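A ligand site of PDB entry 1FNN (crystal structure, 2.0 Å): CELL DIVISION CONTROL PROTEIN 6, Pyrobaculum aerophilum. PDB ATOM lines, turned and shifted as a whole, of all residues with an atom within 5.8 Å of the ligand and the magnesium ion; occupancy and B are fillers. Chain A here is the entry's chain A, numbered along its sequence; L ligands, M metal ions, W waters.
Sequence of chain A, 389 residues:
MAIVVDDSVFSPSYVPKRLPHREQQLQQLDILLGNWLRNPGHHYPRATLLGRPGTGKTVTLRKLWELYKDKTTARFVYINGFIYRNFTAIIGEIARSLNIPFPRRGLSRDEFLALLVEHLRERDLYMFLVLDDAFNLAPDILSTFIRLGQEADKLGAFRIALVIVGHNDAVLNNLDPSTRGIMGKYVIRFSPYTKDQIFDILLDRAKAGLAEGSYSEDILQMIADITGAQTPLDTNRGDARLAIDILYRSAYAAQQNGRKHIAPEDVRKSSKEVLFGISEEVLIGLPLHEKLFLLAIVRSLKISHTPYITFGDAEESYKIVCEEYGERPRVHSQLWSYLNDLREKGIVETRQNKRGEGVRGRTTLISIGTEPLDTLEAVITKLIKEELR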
ATOM      1  N   SER A  11      16.245 -10.270 -17.000  1.00  0.00           N
ATOM      2  CA  SER A  11      15.393  -9.135 -17.393  1.00  0.00           C
ATOM      3  C   SER A  11      16.203  -7.856 -17.362  1.00  0.00           C
ATOM      4  O   SER A  11      17.195  -7.703 -16.638  1.00  0.00           O
ATOM      5  CB  SER A  11      14.154  -8.975 -16.495  1.00  0.00           C
ATOM      6  OG  SER A  11      14.685  -8.774 -15.200  1.00  0.00           O
ATOM      7  N   PRO A  12      15.758  -6.884 -18.150  1.00  0.00           N
ATOM      8  CA  PRO A  12      16.380  -5.581 -18.265  1.00  0.00           C
ATOM      9  C   PRO A  12      16.629  -4.876 -16.950  1.00  0.00           C
ATOM     10  O   PRO A  12      17.625  -4.185 -16.806  1.00  0.00           O
ATOM     11  CB  PRO A  12      15.332  -4.734 -19.022  1.00  0.00           C
ATOM     12  CG  PRO A  12      14.626  -5.753 -19.868  1.00  0.00           C
ATOM     13  CD  PRO A  12      14.534  -6.980 -18.979  1.00  0.00           C
ATOM     14  N   TYR A  14      17.111  -6.292 -13.958  1.00  0.00           N
ATOM     15  CA  TYR A  14      18.025  -6.925 -13.017  1.00  0.00           C
ATOM     16  C   TYR A  14      19.333  -6.170 -12.896  1.00  0.00           C
ATOM     17  O   TYR A  14      19.997  -5.822 -13.892  1.00  0.00           O
ATOM     18  CB  TYR A  14      18.326  -8.349 -13.513  1.00  0.00           C
ATOM     19  CG  TYR A  14      19.261  -9.161 -12.662  1.00  0.00           C
ATOM     20  CD1 TYR A  14      18.745  -9.800 -11.503  1.00  0.00           C
ATOM     21  CD2 TYR A  14      20.590  -9.322 -12.965  1.00  0.00           C
ATOM     22  CE1 TYR A  14      19.602 -10.553 -10.724  1.00  0.00           C
ATOM     23  CE2 TYR A  14      21.439 -10.080 -12.184  1.00  0.00           C
ATOM     24  CZ  TYR A  14      20.902 -10.693 -11.040  1.00  0.00           C
ATOM     25  OH  TYR A  14      21.739 -11.451 -10.247  1.00  0.00           O
ATOM     26  N   VAL A  15      19.790  -5.982 -11.671  1.00  0.00           N
ATOM     27  CA  VAL A  15      21.031  -5.284 -11.328  1.00  0.00           C
ATOM     28  C   VAL A  15      21.945  -6.332 -10.726  1.00  0.00           C
ATOM     29  O   VAL A  15      21.597  -6.899  -9.695  1.00  0.00           O
ATOM     30  CB  VAL A  15      20.828  -4.138 -10.311  1.00  0.00           C
ATOM     31  CG1 VAL A  15      22.187  -3.526  -9.936  1.00  0.00           C
ATOM     32  CG2 VAL A  15      19.934  -3.040 -10.852  1.00  0.00           C
ATOM     33  N   PRO A  16      22.996  -6.758 -11.416  1.00  0.00           N
ATOM     34  CA  PRO A  16      23.808  -7.860 -10.952  1.00  0.00           C
ATOM     35  C   PRO A  16      24.634  -7.416  -9.756  1.00  0.00           C
ATOM     36  O   PRO A  16      24.827  -6.217  -9.533  1.00  0.00           O
ATOM     37  CB  PRO A  16      24.634  -8.245 -12.179  1.00  0.00           C
ATOM     38  CG  PRO A  16      24.660  -7.004 -13.004  1.00  0.00           C
ATOM     39  CD  PRO A  16      23.437  -6.178 -12.719  1.00  0.00           C
ATOM     40  N   ARG A  18      27.933  -7.810  -9.406  1.00  0.00           N
ATOM     41  CA  ARG A  18      29.102  -7.089  -9.875  1.00  0.00           C
ATOM     42  C   ARG A  18      28.901  -6.627 -11.311  1.00  0.00           C
ATOM     43  O   ARG A  18      28.033  -7.093 -12.083  1.00  0.00           O
ATOM     44  CB  ARG A  18      30.367  -7.926  -9.618  1.00  0.00           C
ATOM     45  CG  ARG A  18      30.193  -9.370 -10.027  1.00  0.00           C
ATOM     46  CD  ARG A  18      30.498 -10.309  -8.873  1.00  0.00           C
ATOM     47  NE  ARG A  18      29.524 -11.400  -8.817  1.00  0.00           N
ATOM     48  CZ  ARG A  18      29.546 -12.493  -9.572  1.00  0.00           C
ATOM     49  NH1 ARG A  18      30.522 -12.682 -10.454  1.00  0.00           N
ATOM     50  NH2 ARG A  18      28.593 -13.391  -9.413  1.00  0.00           N
ATOM     51  N   LEU A  19      29.637  -5.599 -11.633  1.00  0.00           N
ATOM     52  CA  LEU A  19      29.720  -4.919 -12.911  1.00  0.00           C
ATOM     53  C   LEU A  19      31.177  -4.978 -13.383  1.00  0.00           C
ATOM     54  O   LEU A  19      31.892  -3.979 -13.458  1.00  0.00           O
ATOM     55  CB  LEU A  19      29.220  -3.485 -12.835  1.00  0.00           C
ATOM     56  CG  LEU A  19      27.754  -3.203 -12.507  1.00  0.00           C
ATOM     57  CD1 LEU A  19      27.441  -1.707 -12.564  1.00  0.00           C
ATOM     58  CD2 LEU A  19      26.754  -3.965 -13.380  1.00  0.00           C
ATOM     59  N   PRO A  20      31.565  -6.141 -13.936  1.00  0.00           N
ATOM     60  CA  PRO A  20      32.931  -6.313 -14.411  1.00  0.00           C
ATOM     61  C   PRO A  20      33.139  -5.353 -15.537  1.00  0.00           C
ATOM     62  O   PRO A  20      32.252  -5.145 -16.374  1.00  0.00           O
ATOM     63  CB  PRO A  20      33.020  -7.787 -14.800  1.00  0.00           C
ATOM     64  CG  PRO A  20      31.600  -8.209 -15.046  1.00  0.00           C
ATOM     65  CD  PRO A  20      30.819  -7.407 -13.989  1.00  0.00           C
ATOM     66  N   HIS A  21      34.312  -4.738 -15.616  1.00  0.00           N
ATOM     67  CA  HIS A  21      34.704  -3.811 -16.667  1.00  0.00           C
ATOM     68  C   HIS A  21      34.066  -2.445 -16.500  1.00  0.00           C
ATOM     69  O   HIS A  21      34.284  -1.585 -17.350  1.00  0.00           O
ATOM     70  CB  HIS A  21      34.516  -4.429 -18.079  1.00  0.00           C
ATOM     71  CG  HIS A  21      35.261  -5.748 -18.110  1.00  0.00           C
ATOM     72  ND1 HIS A  21      36.633  -5.874 -18.082  1.00  0.00           N
ATOM     73  CD2 HIS A  21      34.747  -7.009 -18.175  1.00  0.00           C
ATOM     74  CE1 HIS A  21      36.929  -7.161 -18.127  1.00  0.00           C
ATOM     75  NE2 HIS A  21      35.805  -7.900 -18.179  1.00  0.00           N
ATOM     76  N   ARG A  22      33.333  -2.191 -15.403  1.00  0.00           N
ATOM     77  CA  ARG A  22      32.766  -0.846 -15.190  1.00  0.00           C
ATOM     78  C   ARG A  22      33.229  -0.276 -13.864  1.00  0.00           C
ATOM     79  O   ARG A  22      32.690   0.698 -13.338  1.00  0.00           O
ATOM     80  CB  ARG A  22      31.240  -0.852 -15.230  1.00  0.00           C
ATOM     81  CG  ARG A  22      30.643  -1.101 -16.638  1.00  0.00           C
ATOM     82  CD  ARG A  22      31.035   0.060 -17.507  1.00  0.00           C
ATOM     83  NE  ARG A  22      30.784   0.120 -18.915  1.00  0.00           N
ATOM     84  CZ  ARG A  22      31.734  -0.026 -19.850  1.00  0.00           C
ATOM     85  NH1 ARG A  22      32.983  -0.249 -19.490  1.00  0.00           N
ATOM     86  NH2 ARG A  22      31.377   0.051 -21.114  1.00  0.00           N
ATOM     87  N   GLY A  51      27.858   6.954 -24.159  1.00  0.00           N
ATOM     88  CA  GLY A  51      28.217   5.636 -24.668  1.00  0.00           C
ATOM     89  C   GLY A  51      27.057   5.113 -25.503  1.00  0.00           C
ATOM     90  O   GLY A  51      25.913   5.525 -25.234  1.00  0.00           O
ATOM     91  N   ARG A  52      27.376   4.172 -26.393  1.00  0.00           N
ATOM     92  CA  ARG A  52      26.271   3.641 -27.238  1.00  0.00           C
ATOM     93  C   ARG A  52      25.328   2.786 -26.373  1.00  0.00           C
ATOM     94  O   ARG A  52      25.631   2.422 -25.234  1.00  0.00           O
ATOM     95  CB  ARG A  52      26.853   2.790 -28.374  1.00  0.00           C
ATOM     96  CG  ARG A  52      27.640   1.564 -27.946  1.00  0.00           C
ATOM     97  CD  ARG A  52      27.247   0.303 -28.717  1.00  0.00           C
ATOM     98  NE  ARG A  52      25.787   0.170 -28.872  1.00  0.00           N
ATOM     99  CZ  ARG A  52      25.201  -0.729 -29.650  1.00  0.00           C
ATOM    100  NH1 ARG A  52      26.012  -1.554 -30.317  1.00  0.00           N
ATOM    101  NH2 ARG A  52      23.893  -0.844 -29.791  1.00  0.00           N
ATOM    102  N   PRO A  53      24.261   2.309 -26.997  1.00  0.00           N
ATOM    103  CA  PRO A  53      23.298   1.451 -26.302  1.00  0.00           C
ATOM    104  C   PRO A  53      23.959   0.185 -25.813  1.00  0.00           C
ATOM    105  O   PRO A  53      24.833  -0.430 -26.434  1.00  0.00           O
ATOM    106  CB  PRO A  53      22.190   1.201 -27.308  1.00  0.00           C
ATOM    107  CG  PRO A  53      22.294   2.350 -28.257  1.00  0.00           C
ATOM    108  CD  PRO A  53      23.768   2.657 -28.346  1.00  0.00           C
ATOM    109  N   GLY A  54      23.645  -0.134 -24.544  1.00  0.00           N
ATOM    110  CA  GLY A  54      24.086  -1.416 -24.015  1.00  0.00           C
ATOM    111  C   GLY A  54      25.471  -1.407 -23.407  1.00  0.00           C
ATOM    112  O   GLY A  54      25.979  -2.502 -23.120  1.00  0.00           O
ATOM    113  N   THR A  55      26.017  -0.216 -23.200  1.00  0.00           N
ATOM    114  CA  THR A  55      27.361  -0.121 -22.608  1.00  0.00           C
ATOM    115  C   THR A  55      27.270   0.049 -21.077  1.00  0.00           C
ATOM    116  O   THR A  55      28.321   0.191 -20.457  1.00  0.00           O
ATOM    117  CB  THR A  55      28.162   1.025 -23.208  1.00  0.00           C
ATOM    118  OG1 THR A  55      27.441   2.285 -23.228  1.00  0.00           O
ATOM    119  CG2 THR A  55      28.495   0.691 -24.675  1.00  0.00           C
ATOM    120  N   GLY A  56      26.129  -0.239 -20.437  1.00  0.00           N
ATOM    121  CA  GLY A  56      26.078  -0.217 -18.956  1.00  0.00           C
ATOM    122  C   GLY A  56      25.895   1.159 -18.312  1.00  0.00           C
ATOM    123  O   GLY A  56      26.155   1.323 -17.102  1.00  0.00           O
ATOM    124  N   LYS A  57      25.426   2.160 -19.022  1.00  0.00           N
ATOM    125  CA  LYS A  57      25.259   3.486 -18.436  1.00  0.00           C
ATOM    126  C   LYS A  57      24.193   3.434 -17.311  1.00  0.00           C
ATOM    127  O   LYS A  57      24.458   3.795 -16.189  1.00  0.00           O
ATOM    128  CB  LYS A  57      24.936   4.516 -19.498  1.00  0.00           C
ATOM    129  CG  LYS A  57      25.966   4.591 -20.675  1.00  0.00           C
ATOM    130  CD  LYS A  57      25.569   5.646 -21.690  1.00  0.00           C
ATOM    131  CE  LYS A  57      24.212   5.399 -22.374  1.00  0.00           C
ATOM    132  NZ  LYS A  57      24.321   4.174 -23.216  1.00  0.00           N
ATOM    133  N   THR A  58      22.991   2.943 -17.614  1.00  0.00           N
ATOM    134  CA  THR A  58      21.899   2.897 -16.658  1.00  0.00           C
ATOM    135  C   THR A  58      22.226   1.977 -15.517  1.00  0.00           C
ATOM    136  O   THR A  58      22.040   2.351 -14.329  1.00  0.00           O
ATOM    137  CB  THR A  58      20.587   2.391 -17.319  1.00  0.00           C
ATOM    138  OG1 THR A  58      20.245   3.377 -18.299  1.00  0.00           O
ATOM    139  CG2 THR A  58      19.428   2.259 -16.305  1.00  0.00           C
ATOM    140  N   VAL A  59      22.782   0.796 -15.837  1.00  0.00           N
ATOM    141  CA  VAL A  59      23.070  -0.150 -14.762  1.00  0.00           C
ATOM    142  C   VAL A  59      24.138   0.411 -13.826  1.00  0.00           C
ATOM    143  O   VAL A  59      24.078   0.146 -12.611  1.00  0.00           O
ATOM    144  CB  VAL A  59      23.454  -1.561 -15.212  1.00  0.00           C
ATOM    145  CG1 VAL A  59      24.886  -1.723 -15.698  1.00  0.00           C
ATOM    146  CG2 VAL A  59      23.184  -2.534 -14.065  1.00  0.00           C
ATOM    147  N   THR A  60      25.134   1.099 -14.377  1.00  0.00           N
ATOM    148  CA  THR A  60      26.210   1.665 -13.554  1.00  0.00           C
ATOM    149  C   THR A  60      25.667   2.709 -12.553  1.00  0.00           C
ATOM    150  O   THR A  60      25.972   2.708 -11.355  1.00  0.00           O
ATOM    151  CB  THR A  60      27.316   2.244 -14.451  1.00  0.00           C
ATOM    152  OG1 THR A  60      27.978   1.089 -15.065  1.00  0.00           O
ATOM    153  CG2 THR A  60      28.319   3.029 -13.617  1.00  0.00           C
ATOM    154  N   TYR A  78      14.589   9.305 -10.754  1.00  0.00           N
ATOM    155  CA  TYR A  78      15.049   8.776 -12.056  1.00  0.00           C
ATOM    156  C   TYR A  78      14.063   9.142 -13.148  1.00  0.00           C
ATOM    157  O   TYR A  78      12.886   8.760 -13.120  1.00  0.00           O
ATOM    158  CB  TYR A  78      15.258   7.270 -11.888  1.00  0.00           C
ATOM    159  CG  TYR A  78      15.643   6.633 -13.226  1.00  0.00           C
ATOM    160  CD1 TYR A  78      16.965   6.601 -13.630  1.00  0.00           C
ATOM    161  CD2 TYR A  78      14.641   6.106 -14.039  1.00  0.00           C
ATOM    162  CE1 TYR A  78      17.314   6.036 -14.842  1.00  0.00           C
ATOM    163  CE2 TYR A  78      14.977   5.522 -15.261  1.00  0.00           C
ATOM    164  CZ  TYR A  78      16.318   5.500 -15.647  1.00  0.00           C
ATOM    165  OH  TYR A  78      16.651   4.944 -16.836  1.00  0.00           O
ATOM    166  N   ASP A 132      17.956  10.179 -17.818  1.00  0.00           N
ATOM    167  CA  ASP A 132      18.478   9.093 -18.635  1.00  0.00           C
ATOM    168  C   ASP A 132      17.981   9.245 -20.071  1.00  0.00           C
ATOM    169  O   ASP A 132      16.975   9.902 -20.319  1.00  0.00           O
ATOM    170  CB  ASP A 132      18.041   7.712 -18.112  1.00  0.00           C
ATOM    171  CG  ASP A 132      19.066   6.646 -18.399  1.00  0.00           C
ATOM    172  OD1 ASP A 132      19.962   6.872 -19.274  1.00  0.00           O
ATOM    173  OD2 ASP A 132      19.028   5.574 -17.763  1.00  0.00           O
ATOM    174  N   ASP A 133      18.778   8.779 -21.013  1.00  0.00           N
ATOM    175  CA  ASP A 133      18.507   8.965 -22.437  1.00  0.00           C
ATOM    176  C   ASP A 133      17.989  10.357 -22.749  1.00  0.00           C
ATOM    177  O   ASP A 133      16.961  10.515 -23.411  1.00  0.00           O
ATOM    178  CB  ASP A 133      17.515   7.928 -22.986  1.00  0.00           C
ATOM    179  CG  ASP A 133      18.103   6.549 -22.737  1.00  0.00           C
ATOM    180  OD1 ASP A 133      19.341   6.404 -22.889  1.00  0.00           O
ATOM    181  OD2 ASP A 133      17.274   5.685 -22.385  1.00  0.00           O
ATOM    182  N   VAL A 165      22.381  11.575 -19.415  1.00  0.00           N
ATOM    183  CA  VAL A 165      22.868  10.433 -20.149  1.00  0.00           C
ATOM    184  C   VAL A 165      22.605  10.542 -21.652  1.00  0.00           C
ATOM    185  O   VAL A 165      21.534  10.919 -22.085  1.00  0.00           O
ATOM    186  CB  VAL A 165      22.211   9.145 -19.628  1.00  0.00           C
ATOM    187  CG1 VAL A 165      22.755   7.923 -20.378  1.00  0.00           C
ATOM    188  CG2 VAL A 165      22.400   8.913 -18.141  1.00  0.00           C
ATOM    189  N   TYR A 193      31.664  -2.747 -25.319  1.00  0.00           N
ATOM    190  CA  TYR A 193      32.400  -3.818 -24.675  1.00  0.00           C
ATOM    191  C   TYR A 193      33.117  -4.672 -25.756  1.00  0.00           C
ATOM    192  O   TYR A 193      32.535  -4.948 -26.811  1.00  0.00           O
ATOM    193  CB  TYR A 193      31.494  -4.775 -23.908  1.00  0.00           C
ATOM    194  CG  TYR A 193      30.861  -4.158 -22.668  1.00  0.00           C
ATOM    195  CD1 TYR A 193      29.508  -3.853 -22.594  1.00  0.00           C
ATOM    196  CD2 TYR A 193      31.653  -3.919 -21.553  1.00  0.00           C
ATOM    197  CE1 TYR A 193      28.932  -3.298 -21.452  1.00  0.00           C
ATOM    198  CE2 TYR A 193      31.109  -3.369 -20.396  1.00  0.00           C
ATOM    199  CZ  TYR A 193      29.752  -3.069 -20.373  1.00  0.00           C
ATOM    200  OH  TYR A 193      29.272  -2.517 -19.188  1.00  0.00           O
ATOM    201  N   ILE A 201      30.693 -10.755 -18.630  1.00  0.00           N
ATOM    202  CA  ILE A 201      29.321 -10.410 -18.284  1.00  0.00           C
ATOM    203  C   ILE A 201      28.409 -11.617 -18.413  1.00  0.00           C
ATOM    204  O   ILE A 201      27.595 -11.950 -17.521  1.00  0.00           O
ATOM    205  CB  ILE A 201      28.824  -9.281 -19.162  1.00  0.00           C
ATOM    206  CG1 ILE A 201      29.687  -8.040 -18.827  1.00  0.00           C
ATOM    207  CG2 ILE A 201      27.320  -9.007 -18.980  1.00  0.00           C
ATOM    208  CD1 ILE A 201      29.402  -6.851 -19.751  1.00  0.00           C
ATOM    209  N   ARG A 205      25.966 -13.874 -15.684  1.00  0.00           N
ATOM    210  CA  ARG A 205      24.571 -14.188 -15.886  1.00  0.00           C
ATOM    211  C   ARG A 205      24.310 -15.685 -15.925  1.00  0.00           C
ATOM    212  O   ARG A 205      23.282 -16.175 -15.363  1.00  0.00           O
ATOM    213  CB  ARG A 205      23.959 -13.545 -17.148  1.00  0.00           C
ATOM    214  CG  ARG A 205      24.143 -12.009 -17.193  1.00  0.00           C
ATOM    215  CD  ARG A 205      23.213 -11.357 -16.110  1.00  0.00           C
ATOM    216  NE  ARG A 205      23.610  -9.934 -16.030  1.00  0.00           N
ATOM    217  CZ  ARG A 205      22.738  -8.956 -16.217  1.00  0.00           C
ATOM    218  NH1 ARG A 205      21.464  -9.193 -16.497  1.00  0.00           N
ATOM    219  NH2 ARG A 205      23.175  -7.705 -16.128  1.00  0.00           N
ATOM    220  N   ASP A 239      27.316  -4.254 -27.440  1.00  0.00           N
ATOM    221  CA  ASP A 239      26.075  -4.086 -26.703  1.00  0.00           C
ATOM    222  C   ASP A 239      25.772  -5.258 -25.780  1.00  0.00           C
ATOM    223  O   ASP A 239      25.485  -6.381 -26.203  1.00  0.00           O
ATOM    224  CB  ASP A 239      24.950  -3.894 -27.732  1.00  0.00           C
ATOM    225  CG  ASP A 239      23.587  -3.621 -27.138  1.00  0.00           C
ATOM    226  OD1 ASP A 239      23.325  -4.064 -25.991  1.00  0.00           O
ATOM    227  OD2 ASP A 239      22.782  -2.954 -27.811  1.00  0.00           O
ATOM    228  N   ALA A 240      25.881  -5.054 -24.447  1.00  0.00           N
ATOM    229  CA  ALA A 240      25.657  -6.125 -23.501  1.00  0.00           C
ATOM    230  C   ALA A 240      24.194  -6.529 -23.391  1.00  0.00           C
ATOM    231  O   ALA A 240      23.877  -7.683 -23.066  1.00  0.00           O
ATOM    232  CB  ALA A 240      26.164  -5.723 -22.115  1.00  0.00           C
ATOM    233  N   ARG A 241      23.291  -5.613 -23.689  1.00  0.00           N
ATOM    234  CA  ARG A 241      21.875  -5.991 -23.657  1.00  0.00           C
ATOM    235  C   ARG A 241      21.631  -7.122 -24.661  1.00  0.00           C
ATOM    236  O   ARG A 241      20.872  -8.096 -24.494  1.00  0.00           O
ATOM    237  CB  ARG A 241      21.023  -4.760 -23.981  1.00  0.00           C
ATOM    238  CG  ARG A 241      19.535  -5.042 -23.765  1.00  0.00           C
ATOM    239  CD  ARG A 241      18.610  -4.056 -24.411  1.00  0.00           C
ATOM    240  NE  ARG A 241      18.695  -3.999 -25.851  1.00  0.00           N
ATOM    241  CZ  ARG A 241      18.413  -4.897 -26.788  1.00  0.00           C
ATOM    242  NH1 ARG A 241      17.951  -6.125 -26.544  1.00  0.00           N
ATOM    243  NH2 ARG A 241      18.596  -4.536 -28.049  1.00  0.00           N
ATOM    244  N   ILE A 244      23.124 -10.443 -23.675  1.00  0.00           N
ATOM    245  CA  ILE A 244      22.321 -11.172 -22.643  1.00  0.00           C
ATOM    246  C   ILE A 244      21.013 -11.668 -23.222  1.00  0.00           C
ATOM    247  O   ILE A 244      20.499 -12.752 -22.947  1.00  0.00           O
ATOM    248  CB  ILE A 244      22.092 -10.210 -21.431  1.00  0.00           C
ATOM    249  CG1 ILE A 244      23.446  -9.898 -20.773  1.00  0.00           C
ATOM    250  CG2 ILE A 244      21.103 -10.884 -20.462  1.00  0.00           C
ATOM    251  CD1 ILE A 244      23.470  -8.655 -19.862  1.00  0.00           C
HETATM  252  P1  LIG L   1      22.795   1.312 -21.310  1.00  0.00           P
HETATM  253  O1  LIG L   1      22.011   2.342 -20.519  1.00  0.00           O
HETATM  254  O2  LIG L   1      24.158   1.650 -21.498  1.00  0.00           O
HETATM  255  O3  LIG L   1      22.058   1.293 -22.571  1.00  0.00           O
HETATM  256  P2  LIG L   1      22.405  -0.945 -19.620  1.00  0.00           P
HETATM  257  O4  LIG L   1      22.807  -0.305 -18.359  1.00  0.00           O
HETATM  258  O5  LIG L   1      20.950  -1.104 -19.696  1.00  0.00           O
HETATM  259  O6  LIG L   1      22.951  -0.151 -20.823  1.00  0.00           O
HETATM  260  O7  LIG L   1      23.034  -2.447 -19.766  1.00  0.00           O
HETATM  261  C1  LIG L   1      22.440  -3.270 -20.750  1.00  0.00           C
HETATM  262  C2  LIG L   1      22.278  -4.666 -20.117  1.00  0.00           C
HETATM  263  O8  LIG L   1      23.572  -5.145 -19.806  1.00  0.00           O
HETATM  264  C3  LIG L   1      21.516  -4.691 -18.802  1.00  0.00           C
HETATM  265  O9  LIG L   1      20.855  -5.944 -18.696  1.00  0.00           O
HETATM  266  C4  LIG L   1      22.643  -4.492 -17.845  1.00  0.00           C
HETATM  267  O10 LIG L   1      22.335  -4.965 -16.538  1.00  0.00           O
HETATM  268  C5  LIG L   1      23.715  -5.391 -18.464  1.00  0.00           C
HETATM  269  N1  LIG L   1      24.975  -4.870 -18.108  1.00  0.00           N
HETATM  270  C6  LIG L   1      25.605  -3.817 -18.725  1.00  0.00           C
HETATM  271  N2  LIG L   1      26.851  -3.671 -18.406  1.00  0.00           N
HETATM  272  C7  LIG L   1      27.058  -4.710 -17.517  1.00  0.00           C
HETATM  273  C8  LIG L   1      28.201  -5.097 -16.793  1.00  0.00           C
HETATM  274  N3  LIG L   1      29.332  -4.426 -16.871  1.00  0.00           N
HETATM  275  N4  LIG L   1      28.098  -6.153 -15.980  1.00  0.00           N
HETATM  276  C9  LIG L   1      26.940  -6.786 -15.885  1.00  0.00           C
HETATM  277  N5  LIG L   1      25.790  -6.523 -16.515  1.00  0.00           N
HETATM  278  C10 LIG L   1      25.938  -5.446 -17.335  1.00  0.00           C
HETATM  279 MG    MG M   1      20.260   3.025 -20.391  1.00  0.00          MG
HETATM  280  O   HOH W   1      19.983   2.782 -22.573  1.00  0.00           O
HETATM  281  O   HOH W   2      18.261   3.612 -20.408  1.00  0.00           O
HETATM  282  O   HOH W   3      19.863  -1.247 -17.217  1.00  0.00           O
HETATM  283  O   HOH W   4      19.208   1.119 -19.988  1.00  0.00           O
HETATM  284  O   HOH W   5      20.451  -1.174 -23.486  1.00  0.00           O
HETATM  285  O   HOH W   6      20.239  -3.528 -15.551  1.00  0.00           O
HETATM  286  O   HOH W   7      20.869   4.976 -20.677  1.00  0.00           O
HETATM  287  O   HOH W   8      26.313 -10.133 -15.594  1.00  0.00           O
HETATM  288  O   HOH W   9      18.948  -6.030 -20.508  1.00  0.00           O
HETATM  289  O   HOH W  10      19.597  -6.715 -16.296  1.00  0.00           O
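Water W7 lies within hydrogen-bond range of the side-chain carboxylate (OD1) of Asp 132 (2.5 Å) and the side-chain carboxylate (OD1) of Asp 133 (3.0 Å).
Water W2 lies within hydrogen-bond range of the side-chain carboxylate (OD2) of Asp 133 (3.0 Å) and the side-chain carboxylate (OD2) of Asp 132 (3.4 Å).
Water W6 lies within hydrogen-bond range of an oxygen (O10) of the ligand (2.7 Å), the backbone carbonyl oxygen (O) of Tyr 14 (2.8 Å) and the backbone carbonyl oxygen (O) of Pro 12 (3.0 Å).
Water W8 lies within hydrogen-bond range of the guanidinium group of Arg 205 (2.7 Å) and the backbone carbonyl oxygen of Ile 201 (2.9 Å).
N of Thr 58 lies within hydrogen-bond range of O4 of the ligand (3.3 Å).
O4 of the ligand lies within hydrogen-bond range of N of Val 59 (2.8 Å).
A nitrogen (N2) of the ligand is in hydrogen-bond range of the side-chain hydroxyl of Tyr 193 (2.8 Å).
The backbone NH of Lys 57 is in hydrogen-bond range of an oxygen (O2) of the ligand (2.8 Å).
The side-chain amino group (NZ) of Lys 57 is in salt-bridge range of an oxygen (O2) of the ligand, 3.1 Å away.
N5 of the ligand is in hydrogen-bond range of NH2 of Arg 205, at 2.9 Å.
An oxygen (O3) of the ligand sits at hydrogen-bond distance from the backbone NH (N) of Gly 54 (2.9 Å).
N of Gly 56 lies within hydrogen-bond range of O2 of the ligand.
O of Pro 20 is in hydrogen-bond range of N3 of the ligand (3.0 Å).
An oxygen (O2) of the ligand is in hydrogen-bond range of the backbone NH (N) of Thr 55, 3.1 Å away.
Merely in contact with the ligand: Tyr 14, Pro 16, Arg 18, Leu 19, Arg 22, Pro 53, Ile 201, Ala 240, Arg 241 and Ile 244.
Hydrophobic or aromatic side chains within 4 Å of the ligand: Pro 16, Leu 19, Pro 20, Val 59, Tyr 193, Ile 201, Ala 240 and Ile 244.
Of the 31 residues printed, 19 come within 4 Å of the ligand.
Merely in contact with the magnesium ion: Asp 132 (3.9 Å).
The nearest printed residue that does not touch the magnesium ion is Asp 133 (4.3 Å).
The magnesium ion is bound by O1 of the ligand, water W7, water W2, OG1 of Thr 58, water W1 and water W4.
The magnesium ion has six donor atoms within binding distance.
The side-chain carboxylate of Asp 132 sits close to the side-chain hydroxyl of Thr 58 (2.6 Å).
OH of Tyr 193 is in hydrogen-bond range of O of Thr 55, 3.1 Å away.
NZ of Lys 57 lies within hydrogen-bond range of O of Arg 52, 3.0 Å away.
NZ of Lys 57 is in hydrogen-bond range of O of Gly 51, at 2.9 Å.
The backbone NH of Ala 240 sits at hydrogen-bond distance from the backbone carbonyl oxygen of Gly 54 (2.9 Å).
O of Gly 56 lies within hydrogen-bond range of OG1 of Thr 60, at 2.7 Å.
The backbone carbonyl oxygen of Arg 52 lies within hydrogen-bond range of the side-chain hydroxyl of Thr 55 (2.7 Å).
OD1 of Asp 239 is in hydrogen-bond range of N of Arg 241 (2.8 Å).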
